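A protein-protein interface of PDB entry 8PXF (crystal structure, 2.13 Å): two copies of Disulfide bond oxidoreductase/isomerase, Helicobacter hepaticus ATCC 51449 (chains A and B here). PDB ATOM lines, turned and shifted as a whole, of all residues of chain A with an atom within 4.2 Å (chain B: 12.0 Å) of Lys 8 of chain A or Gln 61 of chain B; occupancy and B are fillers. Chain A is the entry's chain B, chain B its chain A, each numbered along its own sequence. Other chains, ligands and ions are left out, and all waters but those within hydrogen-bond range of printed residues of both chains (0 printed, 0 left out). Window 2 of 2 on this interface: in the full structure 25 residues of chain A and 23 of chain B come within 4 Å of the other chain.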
ATOM      1  N   ALA A   4     -22.432 -33.910  23.167  1.00  0.00           N
ATOM      2  CA  ALA A   4     -22.595 -33.150  21.930  1.00  0.00           C
ATOM      3  C   ALA A   4     -23.042 -31.717  22.219  1.00  0.00           C
ATOM      4  O   ALA A   4     -22.507 -30.755  21.652  1.00  0.00           O
ATOM      5  CB  ALA A   4     -23.596 -33.855  21.016  1.00  0.00           C
ATOM      6  N   GLU A   5     -23.992 -31.550  23.136  1.00  0.00           N
ATOM      7  CA  GLU A   5     -24.382 -30.204  23.535  1.00  0.00           C
ATOM      8  C   GLU A   5     -23.222 -29.495  24.224  1.00  0.00           C
ATOM      9  O   GLU A   5     -23.041 -28.278  24.064  1.00  0.00           O
ATOM     10  CB  GLU A   5     -25.614 -30.281  24.429  1.00  0.00           C
ATOM     11  CG  GLU A   5     -26.876 -30.768  23.688  1.00  0.00           C
ATOM     12  CD  GLU A   5     -27.302 -29.815  22.559  1.00  0.00           C
ATOM     13  OE1 GLU A   5     -27.057 -28.585  22.687  1.00  0.00           O
ATOM     14  OE2 GLU A   5     -27.883 -30.289  21.552  1.00  0.00           O
ATOM     15  N   LEU A   6     -22.394 -30.228  24.962  1.00  0.00           N
ATOM     16  CA  LEU A   6     -21.251 -29.546  25.617  1.00  0.00           C
ATOM     17  C   LEU A   6     -20.343 -28.961  24.551  1.00  0.00           C
ATOM     18  O   LEU A   6     -19.914 -27.830  24.683  1.00  0.00           O
ATOM     19  CB  LEU A   6     -20.453 -30.523  26.473  1.00  0.00           C
ATOM     20  CG  LEU A   6     -20.893 -30.620  27.919  1.00  0.00           C
ATOM     21  CD1 LEU A   6     -20.113 -31.691  28.635  1.00  0.00           C
ATOM     22  CD2 LEU A   6     -20.704 -29.282  28.586  1.00  0.00           C
ATOM     23  N   GLN A   7     -20.128 -29.707  23.487  1.00  0.00           N
ATOM     24  CA  GLN A   7     -19.224 -29.197  22.441  1.00  0.00           C
ATOM     25  C   GLN A   7     -19.818 -27.927  21.849  1.00  0.00           C
ATOM     26  O   GLN A   7     -19.104 -26.955  21.750  1.00  0.00           O
ATOM     27  CB  GLN A   7     -19.067 -30.290  21.401  1.00  0.00           C
ATOM     28  CG  GLN A   7     -17.655 -30.449  20.881  1.00  0.00           C
ATOM     29  CD  GLN A   7     -17.740 -31.269  19.623  1.00  0.00           C
ATOM     30  OE1 GLN A   7     -17.819 -32.487  19.671  1.00  0.00           O
ATOM     31  NE2 GLN A   7     -17.788 -30.596  18.488  1.00  0.00           N
ATOM     32  N   LYS A   8     -21.118 -27.908  21.589  1.00  0.00           N
ATOM     33  CA  LYS A   8     -21.730 -26.698  20.993  1.00  0.00           C
ATOM     34  C   LYS A   8     -21.554 -25.518  21.948  1.00  0.00           C
ATOM     35  O   LYS A   8     -21.243 -24.440  21.481  1.00  0.00           O
ATOM     36  CB  LYS A   8     -23.217 -26.933  20.723  1.00  0.00           C
ATOM     37  CG  LYS A   8     -23.546 -27.834  19.543  1.00  0.00           C
ATOM     38  CD  LYS A   8     -24.976 -28.318  19.536  1.00  0.00           C
ATOM     39  CE  LYS A   8     -25.975 -27.226  19.246  1.00  0.00           C
ATOM     40  NZ  LYS A   8     -27.339 -27.649  19.611  1.00  0.00           N
ATOM     41  N   THR A   9     -21.730 -25.751  23.251  1.00  0.00           N
ATOM     42  CA  THR A   9     -21.594 -24.661  24.255  1.00  0.00           C
ATOM     43  C   THR A   9     -20.161 -24.113  24.261  1.00  0.00           C
ATOM     44  O   THR A   9     -20.010 -22.879  24.260  1.00  0.00           O
ATOM     45  CB  THR A   9     -21.980 -25.164  25.650  1.00  0.00           C
ATOM     46  OG1 THR A   9     -23.340 -25.594  25.599  1.00  0.00           O
ATOM     47  CG2 THR A   9     -21.817 -24.107  26.720  1.00  0.00           C
ATOM     48  N   LEU A  10     -19.154 -24.993  24.226  1.00  0.00           N
ATOM     49  CA  LEU A  10     -17.738 -24.538  24.250  1.00  0.00           C
ATOM     50  C   LEU A  10     -17.434 -23.713  22.996  1.00  0.00           C
ATOM     51  O   LEU A  10     -16.832 -22.632  23.128  1.00  0.00           O
ATOM     52  CB  LEU A  10     -16.832 -25.770  24.304  1.00  0.00           C
ATOM     53  CG  LEU A  10     -16.595 -26.349  25.696  1.00  0.00           C
ATOM     54  CD1 LEU A  10     -15.617 -27.511  25.635  1.00  0.00           C
ATOM     55  CD2 LEU A  10     -16.082 -25.276  26.641  1.00  0.00           C
ATOM     56  N   GLN A  11     -17.871 -24.201  21.835  1.00  0.00           N
ATOM     57  CA  GLN A  11     -17.632 -23.511  20.541  1.00  0.00           C
ATOM     58  C   GLN A  11     -18.367 -22.168  20.499  1.00  0.00           C
ATOM     59  O   GLN A  11     -17.774 -21.191  20.010  1.00  0.00           O
ATOM     60  CB  GLN A  11     -18.122 -24.377  19.381  1.00  0.00           C
ATOM     61  CG  GLN A  11     -17.267 -25.608  19.121  1.00  0.00           C
ATOM     62  CD  GLN A  11     -17.496 -26.143  17.729  1.00  0.00           C
ATOM     63  OE1 GLN A  11     -17.533 -25.396  16.757  1.00  0.00           O
ATOM     64  NE2 GLN A  11     -17.653 -27.452  17.625  1.00  0.00           N
ATOM     65  N   ALA A  12     -19.602 -22.119  21.013  1.00  0.00           N
ATOM     66  CA  ALA A  12     -20.407 -20.876  20.935  1.00  0.00           C
ATOM     67  C   ALA A  12     -19.575 -19.787  21.603  1.00  0.00           C
ATOM     68  O   ALA A  12     -19.513 -18.659  21.080  1.00  0.00           O
ATOM     69  CB  ALA A  12     -21.719 -21.079  21.648  1.00  0.00           C
ATOM     70  N   LYS A  50     -26.138 -27.356  27.978  1.00  0.00           N
ATOM     71  CA  LYS A  50     -26.325 -25.988  27.457  1.00  0.00           C
ATOM     72  C   LYS A  50     -25.651 -24.912  28.310  1.00  0.00           C
ATOM     73  O   LYS A  50     -25.581 -23.794  27.842  1.00  0.00           O
ATOM     74  CB  LYS A  50     -27.808 -25.756  27.202  1.00  0.00           C
ATOM     75  CG  LYS A  50     -28.313 -26.375  25.915  1.00  0.00           C
ATOM     76  CD  LYS A  50     -29.801 -26.535  25.854  1.00  0.00           C
ATOM     77  CE  LYS A  50     -30.235 -27.448  24.732  1.00  0.00           C
ATOM     78  NZ  LYS A  50     -29.680 -27.006  23.436  1.00  0.00           N
ATOM     79  N   LEU B  25     -34.316 -19.618  34.256  1.00  0.00           N
ATOM     80  CA  LEU B  25     -33.264 -19.234  33.328  1.00  0.00           C
ATOM     81  C   LEU B  25     -33.158 -20.181  32.148  1.00  0.00           C
ATOM     82  O   LEU B  25     -32.775 -19.754  31.063  1.00  0.00           O
ATOM     83  CB  LEU B  25     -31.926 -19.167  34.067  1.00  0.00           C
ATOM     84  CG  LEU B  25     -30.689 -18.652  33.347  1.00  0.00           C
ATOM     85  CD1 LEU B  25     -30.936 -17.268  32.801  1.00  0.00           C
ATOM     86  CD2 LEU B  25     -29.529 -18.660  34.335  1.00  0.00           C
ATOM     87  N   GLY B  26     -33.565 -21.437  32.332  1.00  0.00           N
ATOM     88  CA  GLY B  26     -33.394 -22.493  31.363  1.00  0.00           C
ATOM     89  C   GLY B  26     -32.511 -23.599  31.894  1.00  0.00           C
ATOM     90  O   GLY B  26     -31.836 -23.419  32.913  1.00  0.00           O
ATOM     91  N   SER B  27     -32.557 -24.765  31.235  1.00  0.00           N
ATOM     92  CA  SER B  27     -31.667 -25.893  31.538  1.00  0.00           C
ATOM     93  C   SER B  27     -31.732 -26.297  33.015  1.00  0.00           C
ATOM     94  O   SER B  27     -30.741 -26.743  33.600  1.00  0.00           O
ATOM     95  CB  SER B  27     -30.234 -25.585  31.104  1.00  0.00           C
ATOM     96  OG  SER B  27     -30.168 -25.340  29.690  1.00  0.00           O
ATOM     97  N   LEU B  29     -32.236 -24.353  35.632  1.00  0.00           N
ATOM     98  CA  LEU B  29     -31.695 -23.332  36.570  1.00  0.00           C
ATOM     99  C   LEU B  29     -32.589 -22.089  36.560  1.00  0.00           C
ATOM    100  O   LEU B  29     -33.223 -21.824  35.523  1.00  0.00           O
ATOM    101  CB  LEU B  29     -30.268 -22.956  36.156  1.00  0.00           C
ATOM    102  CG  LEU B  29     -29.209 -24.038  36.348  1.00  0.00           C
ATOM    103  CD1 LEU B  29     -27.850 -23.539  35.888  1.00  0.00           C
ATOM    104  CD2 LEU B  29     -29.147 -24.480  37.800  1.00  0.00           C
ATOM    105  N   VAL B  57     -17.561 -17.351  36.673  1.00  0.00           N
ATOM    106  CA  VAL B  57     -17.365 -17.681  35.231  1.00  0.00           C
ATOM    107  C   VAL B  57     -18.609 -18.425  34.736  1.00  0.00           C
ATOM    108  O   VAL B  57     -18.878 -19.530  35.241  1.00  0.00           O
ATOM    109  CB  VAL B  57     -16.091 -18.523  35.023  1.00  0.00           C
ATOM    110  CG1 VAL B  57     -14.861 -17.825  35.580  1.00  0.00           C
ATOM    111  CG2 VAL B  57     -16.229 -19.911  35.625  1.00  0.00           C
ATOM    112  N   LEU B  58     -19.360 -17.820  33.810  1.00  0.00           N
ATOM    113  CA  LEU B  58     -20.573 -18.478  33.254  1.00  0.00           C
ATOM    114  C   LEU B  58     -20.488 -18.519  31.725  1.00  0.00           C
ATOM    115  O   LEU B  58     -20.308 -17.450  31.116  1.00  0.00           O
ATOM    116  CB  LEU B  58     -21.814 -17.701  33.698  1.00  0.00           C
ATOM    117  CG  LEU B  58     -23.128 -18.179  33.085  1.00  0.00           C
ATOM    118  CD1 LEU B  58     -23.603 -19.458  33.756  1.00  0.00           C
ATOM    119  CD2 LEU B  58     -24.196 -17.104  33.183  1.00  0.00           C
ATOM    120  N   ILE B  59     -20.643 -19.708  31.137  1.00  0.00           N
ATOM    121  CA  ILE B  59     -20.619 -19.870  29.653  1.00  0.00           C
ATOM    122  C   ILE B  59     -21.941 -20.525  29.237  1.00  0.00           C
ATOM    123  O   ILE B  59     -22.258 -21.597  29.783  1.00  0.00           O
ATOM    124  CB  ILE B  59     -19.397 -20.702  29.219  1.00  0.00           C
ATOM    125  CG1 ILE B  59     -18.174 -20.395  30.087  1.00  0.00           C
ATOM    126  CG2 ILE B  59     -19.107 -20.501  27.742  1.00  0.00           C
ATOM    127  CD1 ILE B  59     -16.987 -21.286  29.816  1.00  0.00           C
ATOM    128  N   ALA B  60     -22.666 -19.915  28.296  1.00  0.00           N
ATOM    129  CA  ALA B  60     -23.978 -20.450  27.862  1.00  0.00           C
ATOM    130  C   ALA B  60     -24.017 -20.641  26.343  1.00  0.00           C
ATOM    131  O   ALA B  60     -23.611 -19.716  25.618  1.00  0.00           O
ATOM    132  CB  ALA B  60     -25.075 -19.524  28.322  1.00  0.00           C
ATOM    133  N   GLN B  61     -24.523 -21.794  25.893  1.00  0.00           N
ATOM    134  CA  GLN B  61     -24.645 -22.084  24.467  1.00  0.00           C
ATOM    135  C   GLN B  61     -25.286 -20.921  23.727  1.00  0.00           C
ATOM    136  O   GLN B  61     -24.759 -20.437  22.722  1.00  0.00           O
ATOM    137  CB  GLN B  61     -25.467 -23.353  24.268  1.00  0.00           C
ATOM    138  CG  GLN B  61     -25.118 -24.114  23.033  1.00  0.00           C
ATOM    139  CD  GLN B  61     -25.904 -25.404  22.933  1.00  0.00           C
ATOM    140  OE1 GLN B  61     -27.104 -25.399  22.654  1.00  0.00           O
ATOM    141  NE2 GLN B  61     -25.230 -26.519  23.167  1.00  0.00           N
ATOM    142  N   ASP B  62     -26.414 -20.442  24.240  1.00  0.00           N
ATOM    143  CA  ASP B  62     -27.103 -19.274  23.713  1.00  0.00           C
ATOM    144  C   ASP B  62     -26.597 -18.063  24.488  1.00  0.00           C
ATOM    145  O   ASP B  62     -26.821 -17.958  25.700  1.00  0.00           O
ATOM    146  CB  ASP B  62     -28.614 -19.436  23.898  1.00  0.00           C
ATOM    147  CG  ASP B  62     -29.410 -18.205  23.470  1.00  0.00           C
ATOM    148  OD1 ASP B  62     -28.829 -17.289  22.840  1.00  0.00           O
ATOM    149  OD2 ASP B  62     -30.639 -18.180  23.738  1.00  0.00           O
ATOM    150  N   LYS B  63     -25.920 -17.146  23.787  1.00  0.00           N
ATOM    151  CA  LYS B  63     -25.271 -16.031  24.471  1.00  0.00           C
ATOM    152  C   LYS B  63     -26.287 -15.086  25.096  1.00  0.00           C
ATOM    153  O   LYS B  63     -25.983 -14.442  26.106  1.00  0.00           O
ATOM    154  CB  LYS B  63     -24.344 -15.293  23.505  1.00  0.00           C
ATOM    155  CG  LYS B  63     -23.231 -16.187  22.960  1.00  0.00           C
ATOM    156  CD  LYS B  63     -23.097 -16.077  21.449  1.00  0.00           C
ATOM    157  CE  LYS B  63     -24.390 -16.459  20.743  1.00  0.00           C
ATOM    158  NZ  LYS B  63     -24.619 -17.919  20.759  1.00  0.00           N
ATOM    159  N   SER B  64     -27.489 -14.990  24.520  1.00  0.00           N
ATOM    160  CA  SER B  64     -28.527 -14.145  25.100  1.00  0.00           C
ATOM    161  C   SER B  64     -28.767 -14.513  26.559  1.00  0.00           C
ATOM    162  O   SER B  64     -28.919 -13.633  27.417  1.00  0.00           O
ATOM    163  CB  SER B  64     -29.810 -14.242  24.274  1.00  0.00           C
ATOM    164  OG  SER B  64     -30.741 -15.136  24.851  1.00  0.00           O
ATOM    165  N   THR B  65     -28.752 -15.817  26.847  1.00  0.00           N
ATOM    166  CA  THR B  65     -28.976 -16.302  28.234  1.00  0.00           C
ATOM    167  C   THR B  65     -27.869 -15.749  29.137  1.00  0.00           C
ATOM    168  O   THR B  65     -28.191 -15.283  30.243  1.00  0.00           O
ATOM    169  CB  THR B  65     -28.967 -17.834  28.285  1.00  0.00           C
ATOM    170  OG1 THR B  65     -30.180 -18.304  27.699  1.00  0.00           O
ATOM    171  CG2 THR B  65     -28.844 -18.371  29.694  1.00  0.00           C
ATOM    172  N   GLU B  66     -26.624 -15.763  28.654  1.00  0.00           N
ATOM    173  CA  GLU B  66     -25.477 -15.244  29.443  1.00  0.00           C
ATOM    174  C   GLU B  66     -25.691 -13.751  29.706  1.00  0.00           C
ATOM    175  O   GLU B  66     -25.483 -13.317  30.852  1.00  0.00           O
ATOM    176  CB  GLU B  66     -24.184 -15.453  28.657  1.00  0.00           C
ATOM    177  CG  GLU B  66     -23.149 -14.371  28.898  1.00  0.00           C
ATOM    178  CD  GLU B  66     -22.098 -14.265  27.807  1.00  0.00           C
ATOM    179  OE1 GLU B  66     -21.859 -15.278  27.119  1.00  0.00           O
ATOM    180  OE2 GLU B  66     -21.530 -13.168  27.642  1.00  0.00           O
ATOM    181  N   SER B  67     -26.132 -13.012  28.686  1.00  0.00           N
ATOM    182  CA  SER B  67     -26.382 -11.554  28.830  1.00  0.00           C
ATOM    183  C   SER B  67     -27.501 -11.341  29.849  1.00  0.00           C
ATOM    184  O   SER B  67     -27.380 -10.428  30.685  1.00  0.00           O
ATOM    185  CB  SER B  67     -26.748 -10.949  27.505  1.00  0.00           C
ATOM    186  OG  SER B  67     -28.084 -11.278  27.161  1.00  0.00           O
ATOM    187  N   ARG B  68     -28.532 -12.189  29.794  1.00  0.00           N
ATOM    188  CA  ARG B  68     -29.687 -12.073  30.714  1.00  0.00           C
ATOM    189  C   ARG B  68     -29.205 -12.180  32.166  1.00  0.00           C
ATOM    190  O   ARG B  68     -29.720 -11.444  33.004  1.00  0.00           O
ATOM    191  CB  ARG B  68     -30.710 -13.152  30.368  1.00  0.00           C
ATOM    192  CG  ARG B  68     -32.073 -12.907  30.987  1.00  0.00           C
ATOM    193  CD  ARG B  68     -33.059 -13.880  30.399  1.00  0.00           C
ATOM    194  NE  ARG B  68     -34.158 -14.099  31.316  1.00  0.00           N
ATOM    195  CZ  ARG B  68     -34.714 -15.280  31.504  1.00  0.00           C
ATOM    196  NH1 ARG B  68     -34.255 -16.327  30.845  1.00  0.00           N
ATOM    197  NH2 ARG B  68     -35.713 -15.415  32.353  1.00  0.00           N
ATOM    198  N   VAL B  69     -28.259 -13.072  32.451  1.00  0.00           N
ATOM    199  CA  VAL B  69     -27.733 -13.190  33.839  1.00  0.00           C
ATOM    200  C   VAL B  69     -27.048 -11.876  34.218  1.00  0.00           C
ATOM    201  O   VAL B  69     -27.300 -11.390  35.310  1.00  0.00           O
ATOM    202  CB  VAL B  69     -26.769 -14.376  33.971  1.00  0.00           C
ATOM    203  CG1 VAL B  69     -25.986 -14.310  35.263  1.00  0.00           C
ATOM    204  CG2 VAL B  69     -27.499 -15.696  33.859  1.00  0.00           C
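The backbone NH (N) of Gln 61 of chain B is in hydrogen-bond range of the backbone carbonyl oxygen (O) of Lys 50 of chain A (3.0 Å). The side-chain amide nitrogen of Gln 61 of chain B lies within hydrogen-bond range of the side-chain hydroxyl of Thr 9 of chain A (3.2 Å). The side-chain amide nitrogen (NE2) of Gln 61 of chain B sits at hydrogen-bond distance from the side-chain carboxylate (OE1) of Glu 5 of chain A, 2.8 Å away.
OE1 of Glu 5 of chain A is in salt-bridge range of NZ of Lys 50 of chain A (3.2 Å). The backbone carbonyl oxygen of Glu 5 of chain A is in hydrogen-bond range of the side-chain hydroxyl of Thr 9 of chain A, 3.1 Å away. The side-chain carboxylate (OE1) of Glu 5 of chain A is in salt-bridge range of the side-chain amino group (NZ) of Lys 8 of chain A (3.2 Å). O of Gln 61 of chain B sits at hydrogen-bond distance from NZ of Lys 63 of chain B, at 3.2 Å.
Among the printed residues, merely in contact across the chains: Lys 8 of chain A with Gln 61 of chain B, Thr 9 of chain A with Ile 59 of chain B, Ala 12 of chain A with Gln 61 of chain B, Lys 50 of chain A with Ser 27 of chain B and Lys 50 of chain A with Ala 60 of chain B.
No residue of chain B comes within 4 Å of Ala 4 of chain A. No residue of chain B comes within 4 Å of Gln 7 of chain A. Lys 8 of chain A touches one residue of chain B. Of the printed residues of chain B, Thr 9 of chain A touches Ile 59 and Gln 61. No residue of chain B comes within 4 Å of Gln 11 of chain A. Of chain B, only Ser 27, Ala 60 and Gln 61 come within 4 Å of Lys 50 of chain A. Of the printed residues of chain A, Ser 27 of chain B touches Lys 50 (3.5 Å). Ser 64 of chain B touches none of the printed residues of chain A. Arg 68 of chain B touches none of the printed residues of chain A.
Printed residues of chain B that touch a printed residue of chain A: Ser 27, Ile 59, Ala 60 and Gln 61. Along chain B the printed residues that touch a printed residue of chain A span positions 27 to 61. Of the 10 printed residues of chain A, 5 touch a printed residue of chain B. Printed residues of chain A that touch a printed residue of chain B: Glu 5, Lys 8, Thr 9, Ala 12 and Lys 50. Among the printed residues, no Asp or Glu carboxylate lies within 4 Å of a Lys or Arg side-chain nitrogen of the other chain.
No position is printed for both chains.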
